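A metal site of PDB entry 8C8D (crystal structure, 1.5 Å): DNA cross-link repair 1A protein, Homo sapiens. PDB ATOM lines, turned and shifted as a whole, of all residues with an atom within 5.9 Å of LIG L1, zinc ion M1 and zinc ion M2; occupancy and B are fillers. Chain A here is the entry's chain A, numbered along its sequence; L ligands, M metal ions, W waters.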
ATOM      1  N   HIS A  35      24.750  17.140  23.496  1.00  0.00           N
ATOM      2  CA  HIS A  35      26.064  17.480  22.977  1.00  0.00           C
ATOM      3  C   HIS A  35      26.565  18.768  23.618  1.00  0.00           C
ATOM      4  O   HIS A  35      25.789  19.534  24.192  1.00  0.00           O
ATOM      5  CB  HIS A  35      26.104  17.561  21.438  1.00  0.00           C
ATOM      6  CG  HIS A  35      25.299  18.671  20.830  1.00  0.00           C
ATOM      7  ND1 HIS A  35      23.917  18.734  20.886  1.00  0.00           N
ATOM      8  CD2 HIS A  35      25.686  19.734  20.090  1.00  0.00           C
ATOM      9  CE1 HIS A  35      23.496  19.793  20.229  1.00  0.00           C
ATOM     10  NE2 HIS A  35      24.557  20.418  19.724  1.00  0.00           N
ATOM     11  N   HIS A  37      27.377  21.914  22.961  1.00  0.00           N
ATOM     12  CA  HIS A  37      27.224  23.205  22.295  1.00  0.00           C
ATOM     13  C   HIS A  37      26.486  24.152  23.232  1.00  0.00           C
ATOM     14  O   HIS A  37      25.560  23.739  23.932  1.00  0.00           O
ATOM     15  CB  HIS A  37      26.462  23.086  20.969  1.00  0.00           C
ATOM     16  CG  HIS A  37      27.316  22.686  19.808  1.00  0.00           C
ATOM     17  ND1 HIS A  37      26.793  22.208  18.636  1.00  0.00           N
ATOM     18  CD2 HIS A  37      28.664  22.694  19.643  1.00  0.00           C
ATOM     19  CE1 HIS A  37      27.775  21.944  17.791  1.00  0.00           C
ATOM     20  NE2 HIS A  37      28.921  22.228  18.377  1.00  0.00           N
ATOM     21  N   SER A  38      26.879  25.428  23.217  1.00  0.00           N
ATOM     22  CA  SER A  38      26.468  26.349  24.274  1.00  0.00           C
ATOM     23  C   SER A  38      24.955  26.548  24.338  1.00  0.00           C
ATOM     24  O   SER A  38      24.410  26.750  25.435  1.00  0.00           O
ATOM     25  CB  SER A  38      27.194  27.693  24.142  1.00  0.00           C
ATOM     26  OG  SER A  38      26.945  28.285  22.885  1.00  0.00           O
ATOM     27  N   ASP A  39      24.262  26.481  23.201  1.00  0.00           N
ATOM     28  CA  ASP A  39      22.812  26.597  23.209  1.00  0.00           C
ATOM     29  C   ASP A  39      22.125  25.387  23.843  1.00  0.00           C
ATOM     30  O   ASP A  39      20.898  25.409  24.016  1.00  0.00           O
ATOM     31  CB  ASP A  39      22.255  26.868  21.805  1.00  0.00           C
ATOM     32  CG  ASP A  39      22.864  25.970  20.745  1.00  0.00           C
ATOM     33  OD1 ASP A  39      24.093  25.724  20.811  1.00  0.00           O
ATOM     34  OD2 ASP A  39      22.126  25.512  19.850  1.00  0.00           O
ATOM     35  N   HIS A  40      22.885  24.360  24.205  1.00  0.00           N
ATOM     36  CA  HIS A  40      22.336  23.161  24.823  1.00  0.00           C
ATOM     37  C   HIS A  40      22.785  22.957  26.262  1.00  0.00           C
ATOM     38  O   HIS A  40      21.983  22.512  27.091  1.00  0.00           O
ATOM     39  CB  HIS A  40      22.671  21.923  23.989  1.00  0.00           C
ATOM     40  CG  HIS A  40      22.162  22.034  22.582  1.00  0.00           C
ATOM     41  ND1 HIS A  40      21.019  21.389  22.155  1.00  0.00           N
ATOM     42  CD2 HIS A  40      22.603  22.751  21.524  1.00  0.00           C
ATOM     43  CE1 HIS A  40      20.790  21.690  20.900  1.00  0.00           C
ATOM     44  NE2 HIS A  40      21.746  22.517  20.488  1.00  0.00           N
ATOM     45  N   HIS A  96      26.602  14.931  14.251  1.00  0.00           N
ATOM     46  CA  HIS A  96      26.633  16.382  14.446  1.00  0.00           C
ATOM     47  C   HIS A  96      28.087  16.736  14.764  1.00  0.00           C
ATOM     48  O   HIS A  96      28.940  16.658  13.877  1.00  0.00           O
ATOM     49  CB  HIS A  96      25.613  16.772  15.534  1.00  0.00           C
ATOM     50  CG  HIS A  96      25.455  18.244  15.770  1.00  0.00           C
ATOM     51  ND1 HIS A  96      25.171  19.155  14.766  1.00  0.00           N
ATOM     52  CD2 HIS A  96      25.495  18.966  16.918  1.00  0.00           C
ATOM     53  CE1 HIS A  96      25.055  20.363  15.294  1.00  0.00           C
ATOM     54  NE2 HIS A  96      25.254  20.280  16.591  1.00  0.00           N
ATOM     55  N   CYS A  97      28.385  17.086  15.996  1.00  0.00           N
ATOM     56  CA  CYS A  97      29.752  17.358  16.450  1.00  0.00           C
ATOM     57  C   CYS A  97      30.254  16.190  17.298  1.00  0.00           C
ATOM     58  O   CYS A  97      29.486  15.287  17.640  1.00  0.00           O
ATOM     59  CB  CYS A  97      29.771  18.646  17.270  1.00  0.00           C
ATOM     60  SG  CYS A  97      28.851  18.545  18.818  1.00  0.00           S
ATOM     61  N   ASP A 118      20.745  17.755  18.212  1.00  0.00           N
ATOM     62  CA  ASP A 118      21.099  18.275  16.894  1.00  0.00           C
ATOM     63  C   ASP A 118      21.667  17.120  16.070  1.00  0.00           C
ATOM     64  O   ASP A 118      22.486  16.349  16.594  1.00  0.00           O
ATOM     65  CB  ASP A 118      22.173  19.364  16.992  1.00  0.00           C
ATOM     66  CG  ASP A 118      21.628  20.689  17.464  1.00  0.00           C
ATOM     67  OD1 ASP A 118      20.395  20.840  17.610  1.00  0.00           O
ATOM     68  OD2 ASP A 118      22.459  21.597  17.698  1.00  0.00           O
ATOM     69  N   THR A 143      16.328  22.626  12.303  1.00  0.00           N
ATOM     70  CA  THR A 143      17.081  23.845  11.985  1.00  0.00           C
ATOM     71  C   THR A 143      16.854  24.279  10.536  1.00  0.00           C
ATOM     72  O   THR A 143      16.524  25.435  10.279  1.00  0.00           O
ATOM     73  CB  THR A 143      18.581  23.641  12.276  1.00  0.00           C
ATOM     74  OG1 THR A 143      18.756  23.335  13.660  1.00  0.00           O
ATOM     75  CG2 THR A 143      19.374  24.903  11.927  1.00  0.00           C
ATOM     76  N   TYR A 144      17.006  23.364   9.599  1.00  0.00           N
ATOM     77  CA  TYR A 144      16.912  23.697   8.173  1.00  0.00           C
ATOM     78  C   TYR A 144      15.690  23.080   7.503  1.00  0.00           C
ATOM     79  O   TYR A 144      15.761  22.592   6.372  1.00  0.00           O
ATOM     80  CB  TYR A 144      18.194  23.311   7.448  1.00  0.00           C
ATOM     81  CG  TYR A 144      19.382  24.132   7.876  1.00  0.00           C
ATOM     82  CD1 TYR A 144      19.329  25.506   7.910  1.00  0.00           C
ATOM     83  CD2 TYR A 144      20.563  23.509   8.265  1.00  0.00           C
ATOM     84  CE1 TYR A 144      20.412  26.271   8.289  1.00  0.00           C
ATOM     85  CE2 TYR A 144      21.661  24.262   8.658  1.00  0.00           C
ATOM     86  CZ  TYR A 144      21.575  25.647   8.667  1.00  0.00           C
ATOM     87  OH  TYR A 144      22.654  26.408   9.053  1.00  0.00           O
ATOM     88  N   TYR A 182      34.800  28.252  16.802  1.00  0.00           N
ATOM     89  CA  TYR A 182      34.367  28.633  18.139  1.00  0.00           C
ATOM     90  C   TYR A 182      34.038  27.379  18.941  1.00  0.00           C
ATOM     91  O   TYR A 182      34.783  26.990  19.852  1.00  0.00           O
ATOM     92  CB  TYR A 182      33.172  29.599  18.141  1.00  0.00           C
ATOM     93  CG  TYR A 182      32.318  29.635  16.890  1.00  0.00           C
ATOM     94  CD1 TYR A 182      31.862  28.471  16.276  1.00  0.00           C
ATOM     95  CD2 TYR A 182      31.909  30.856  16.347  1.00  0.00           C
ATOM     96  CE1 TYR A 182      31.076  28.519  15.145  1.00  0.00           C
ATOM     97  CE2 TYR A 182      31.121  30.913  15.219  1.00  0.00           C
ATOM     98  CZ  TYR A 182      30.702  29.742  14.622  1.00  0.00           C
ATOM     99  OH  TYR A 182      29.916  29.790  13.491  1.00  0.00           O
ATOM    100  N   SER A 183      32.936  26.737  18.600  1.00  0.00           N
ATOM    101  CA  SER A 183      32.506  25.540  19.311  1.00  0.00           C
ATOM    102  C   SER A 183      33.276  24.335  18.800  1.00  0.00           C
ATOM    103  O   SER A 183      34.078  24.412  17.862  1.00  0.00           O
ATOM    104  CB  SER A 183      31.000  25.347  19.119  1.00  0.00           C
ATOM    105  OG  SER A 183      30.663  25.363  17.748  1.00  0.00           O
ATOM    106  N   ILE A 184      33.033  23.187  19.427  1.00  0.00           N
ATOM    107  CA  ILE A 184      33.477  21.918  18.865  1.00  0.00           C
ATOM    108  C   ILE A 184      32.652  21.642  17.625  1.00  0.00           C
ATOM    109  O   ILE A 184      31.621  22.286  17.393  1.00  0.00           O
ATOM    110  CB  ILE A 184      33.366  20.763  19.876  1.00  0.00           C
ATOM    111  CG1 ILE A 184      31.897  20.566  20.266  1.00  0.00           C
ATOM    112  CG2 ILE A 184      34.247  21.033  21.082  1.00  0.00           C
ATOM    113  CD1 ILE A 184      31.630  19.301  21.084  1.00  0.00           C
ATOM    114  N   LYS A 186      33.119  20.320  13.230  1.00  0.00           N
ATOM    115  CA  LYS A 186      33.745  20.740  11.977  1.00  0.00           C
ATOM    116  C   LYS A 186      35.267  20.627  12.024  1.00  0.00           C
ATOM    117  O   LYS A 186      35.959  21.278  11.237  1.00  0.00           O
ATOM    118  CB  LYS A 186      33.292  22.145  11.563  1.00  0.00           C
ATOM    119  CG  LYS A 186      31.757  22.316  11.626  1.00  0.00           C
ATOM    120  CD  LYS A 186      31.286  23.664  11.074  1.00  0.00           C
ATOM    121  CE  LYS A 186      29.768  23.828  11.267  1.00  0.00           C
ATOM    122  NZ  LYS A 186      29.267  25.064  10.604  1.00  0.00           N
ATOM    123  N   THR A 265      30.896  28.130   7.600  1.00  0.00           N
ATOM    124  CA  THR A 265      29.566  28.567   8.010  1.00  0.00           C
ATOM    125  C   THR A 265      28.560  27.434   7.841  1.00  0.00           C
ATOM    126  O   THR A 265      28.878  26.332   7.391  1.00  0.00           O
ATOM    127  CB  THR A 265      29.127  29.745   7.153  1.00  0.00           C
ATOM    128  OG1 THR A 265      28.903  29.291   5.810  1.00  0.00           O
ATOM    129  CG2 THR A 265      30.199  30.816   7.141  1.00  0.00           C
ATOM    130  N   GLY A 266      27.316  27.719   8.224  1.00  0.00           N
ATOM    131  CA  GLY A 266      26.212  26.839   7.876  1.00  0.00           C
ATOM    132  C   GLY A 266      25.698  27.194   6.488  1.00  0.00           C
ATOM    133  O   GLY A 266      26.491  27.516   5.593  1.00  0.00           O
ATOM    134  N   TRP A 267      24.385  27.150   6.305  1.00  0.00           N
ATOM    135  CA  TRP A 267      23.807  27.594   5.051  1.00  0.00           C
ATOM    136  C   TRP A 267      23.872  29.114   4.948  1.00  0.00           C
ATOM    137  O   TRP A 267      23.705  29.822   5.936  1.00  0.00           O
ATOM    138  CB  TRP A 267      22.350  27.144   4.946  1.00  0.00           C
ATOM    139  CG  TRP A 267      21.580  27.761   3.796  1.00  0.00           C
ATOM    140  CD1 TRP A 267      21.370  27.220   2.555  1.00  0.00           C
ATOM    141  CD2 TRP A 267      20.923  29.043   3.795  1.00  0.00           C
ATOM    142  NE1 TRP A 267      20.624  28.086   1.782  1.00  0.00           N
ATOM    143  CE2 TRP A 267      20.333  29.206   2.518  1.00  0.00           C
ATOM    144  CE3 TRP A 267      20.768  30.062   4.745  1.00  0.00           C
ATOM    145  CZ2 TRP A 267      19.604  30.348   2.168  1.00  0.00           C
ATOM    146  CZ3 TRP A 267      20.042  31.194   4.392  1.00  0.00           C
ATOM    147  CH2 TRP A 267      19.474  31.318   3.121  1.00  0.00           C
ATOM    148  N   HIS A 297      24.164  20.089  10.462  1.00  0.00           N
ATOM    149  CA  HIS A 297      22.723  19.906  10.550  1.00  0.00           C
ATOM    150  C   HIS A 297      22.193  19.372   9.220  1.00  0.00           C
ATOM    151  O   HIS A 297      22.739  19.661   8.157  1.00  0.00           O
ATOM    152  CB  HIS A 297      21.977  21.235  10.848  1.00  0.00           C
ATOM    153  CG  HIS A 297      22.222  21.783  12.224  1.00  0.00           C
ATOM    154  ND1 HIS A 297      21.522  21.349  13.328  1.00  0.00           N
ATOM    155  CD2 HIS A 297      23.051  22.761  12.667  1.00  0.00           C
ATOM    156  CE1 HIS A 297      21.916  22.021  14.400  1.00  0.00           C
ATOM    157  NE2 HIS A 297      22.839  22.893  14.017  1.00  0.00           N
HETATM  158  C1  LIG L   1      27.641  25.117  16.566  1.00  0.00           C
HETATM  159  C2  LIG L   1      22.774  28.852  17.922  1.00  0.00           C
HETATM  160  C3  LIG L   1      22.771  27.642  15.935  1.00  0.00           C
HETATM  161  C4  LIG L   1      22.698  26.421  13.792  1.00  0.00           C
HETATM  162  C5  LIG L   1      23.754  27.057  12.964  1.00  0.00           C
HETATM  163  C6  LIG L   1      23.773  28.197  12.245  1.00  0.00           C
HETATM  164  C7  LIG L   1      25.072  28.302  11.663  1.00  0.00           C
HETATM  165  C8  LIG L   1      25.766  27.193  12.085  1.00  0.00           C
HETATM  166  C9  LIG L   1      25.341  24.336  17.148  1.00  0.00           C
HETATM  167  C10 LIG L   1      26.164  25.519  16.639  1.00  0.00           C
HETATM  168  C11 LIG L   1      25.971  26.757  17.527  1.00  0.00           C
HETATM  169  C12 LIG L   1      24.621  27.396  17.302  1.00  0.00           C
HETATM  170  C13 LIG L   1      24.048  28.313  18.242  1.00  0.00           C
HETATM  171  C14 LIG L   1      24.679  28.679  19.443  1.00  0.00           C
HETATM  172  C15 LIG L   1      24.056  29.563  20.275  1.00  0.00           C
HETATM  173  C16 LIG L   1      22.800  30.110  19.982  1.00  0.00           C
HETATM  174  C17 LIG L   1      22.168  29.752  18.821  1.00  0.00           C
HETATM  175  N1  LIG L   1      22.144  28.507  16.756  1.00  0.00           N
HETATM  176  N2  LIG L   1      22.143  27.308  14.802  1.00  0.00           N
HETATM  177  N3  LIG L   1      23.980  27.080  16.170  1.00  0.00           N
HETATM  178  N4  LIG L   1      24.771  24.491  18.332  1.00  0.00           N
HETATM  179  O1  LIG L   1      24.960  26.418  12.883  1.00  0.00           O
HETATM  180  O2  LIG L   1      24.049  23.440  18.889  1.00  0.00           O
HETATM  181  O3  LIG L   1      25.219  23.304  16.486  1.00  0.00           O
HETATM  182 CL1  LIG L   1      24.821  30.031  21.766  1.00  0.00          CL
HETATM  183  C1  LG2 L   2      28.860  32.681  18.379  1.00  0.00           C
HETATM  184  C2  LG2 L   2      24.419  31.268  16.377  1.00  0.00           C
HETATM  185  C3  LG2 L   2      23.422  32.779  17.852  1.00  0.00           C
HETATM  186  C4  LG2 L   2      21.934  33.795  19.504  1.00  0.00           C
HETATM  187  C5  LG2 L   2      22.734  34.804  20.247  1.00  0.00           C
HETATM  188  C6  LG2 L   2      23.422  35.885  19.861  1.00  0.00           C
HETATM  189  C7  LG2 L   2      23.970  36.466  21.037  1.00  0.00           C
HETATM  190  C8  LG2 L   2      23.554  35.695  22.081  1.00  0.00           C
HETATM  191  C9  LG2 L   2      26.983  34.323  18.499  1.00  0.00           C
HETATM  192  C10 LG2 L   2      27.648  33.144  19.195  1.00  0.00           C
HETATM  193  C11 LG2 L   2      26.641  31.989  19.439  1.00  0.00           C
HETATM  194  C12 LG2 L   2      25.512  31.983  18.439  1.00  0.00           C
HETATM  195  C13 LG2 L   2      25.541  31.188  17.243  1.00  0.00           C
HETATM  196  C14 LG2 L   2      26.620  30.353  16.892  1.00  0.00           C
HETATM  197  C15 LG2 L   2      26.560  29.639  15.736  1.00  0.00           C
HETATM  198  C16 LG2 L   2      25.460  29.703  14.875  1.00  0.00           C
HETATM  199  C17 LG2 L   2      24.405  30.513  15.189  1.00  0.00           C
HETATM  200  N1  LG2 L   2      23.355  32.077  16.686  1.00  0.00           N
HETATM  201  N2  LG2 L   2      22.379  33.565  18.149  1.00  0.00           N
HETATM  202  N3  LG2 L   2      24.462  32.754  18.711  1.00  0.00           N
HETATM  203  N4  LG2 L   2      26.514  35.280  19.279  1.00  0.00           N
HETATM  204  O1  LG2 L   2      22.782  34.667  21.607  1.00  0.00           O
HETATM  205  O2  LG2 L   2      26.641  35.191  20.658  1.00  0.00           O
HETATM  206  O3  LG2 L   2      26.908  34.362  17.275  1.00  0.00           O
HETATM  207 CL1  LG2 L   2      27.884  28.599  15.295  1.00  0.00          CL
HETATM  208 ZN    ZN M   1      24.817  21.749  18.072  1.00  0.00          ZN
HETATM  209 ZN    ZN M   2      22.042  23.469  18.628  1.00  0.00          ZN
HETATM  210  O   HOH W   1      26.527  23.240  13.922  1.00  0.00           O
HETATM  211  O   HOH W   2      19.829  24.965  15.681  1.00  0.00           O
HETATM  212  O   HOH W   3      24.754  24.890   9.872  1.00  0.00           O
HETATM  213  O   HOH W   4      20.038  23.343  18.089  1.00  0.00           O
HETATM  214  O   HOH W   5      22.373  24.426  16.689  1.00  0.00           O
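The backbone carbonyl oxygen (O) of Ile 184 lies within hydrogen-bond range of a ring nitrogen (NE2) of His 37 (2.9 Å).
The side-chain sulfur (SG) of Cys 97 sits close to a ring nitrogen (NE2) of His 37, at 3.7 Å.
ND1 of His 297 is in hydrogen-bond range of OG1 of Thr 143 (3.4 Å).
The side-chain hydroxyl of Tyr 144 sits at hydrogen-bond distance from the backbone NH of Trp 267, at 3.3 Å.
Merely in contact with LIG L1: Ser 38, Tyr 144 and Ser 183.
Ten residues have an atom within 4 Å of LIG L1: His 35, His 37, Ser 38, Asp 39, His 40, His 96, Asp 118, Tyr 144, Ser 183 and His 297.
A ring nitrogen (NE2) of His 297 lies close to an oxygen (O3) of LIG L1 (3.5 Å).
Within 4 Å of zinc ion M2: Asp 39, His 40 and Asp 118.
An oxygen (O2) of LIG L1 is bound to zinc ion M2, at 2.0 Å.
Water W4 binds zinc ion M2, 2.1 Å away.
NE2 of His 40 is bound to zinc ion M2 (2.1 Å).
OD2 of Asp 118 binds zinc ion M2, 2.1 Å away.
Water W5 binds zinc ion M2 (2.2 Å).
Zinc ion M2 is bound by the side-chain carboxylate (OD2) of Asp 39.
Water W5 bridges N4 of LIG L1 (2.9 Å) and NE2 of His 297 (3.1 Å).
Water W3 lies within hydrogen-bond range of OH of Tyr 144 (2.7 Å) and O1 of LIG L1 (3.4 Å).
Water W2 bridges OG1 of Thr 143 (2.8 Å) and N2 of LIG L1 (3.4 Å).
Five residues have an atom within 4 Å of zinc ion M1: His 35, His 37, His 40, His 96 and Asp 118.
An oxygen (O2) of LIG L1 is bound to zinc ion M1, 2.0 Å away.
ND1 of His 37 binds zinc ion M1 (2.1 Å).
Zinc ion M1 is bound by NE2 of His 96 (2.1 Å).
A ring nitrogen (NE2) of His 35 binds zinc ion M1, 2.1 Å away.
O3 of LIG L1 binds zinc ion M1 (2.3 Å).
Zinc ion M1 is bound by OD2 of Asp 118, 2.4 Å away.
Zinc ion M1 has six donor atoms within binding distance.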
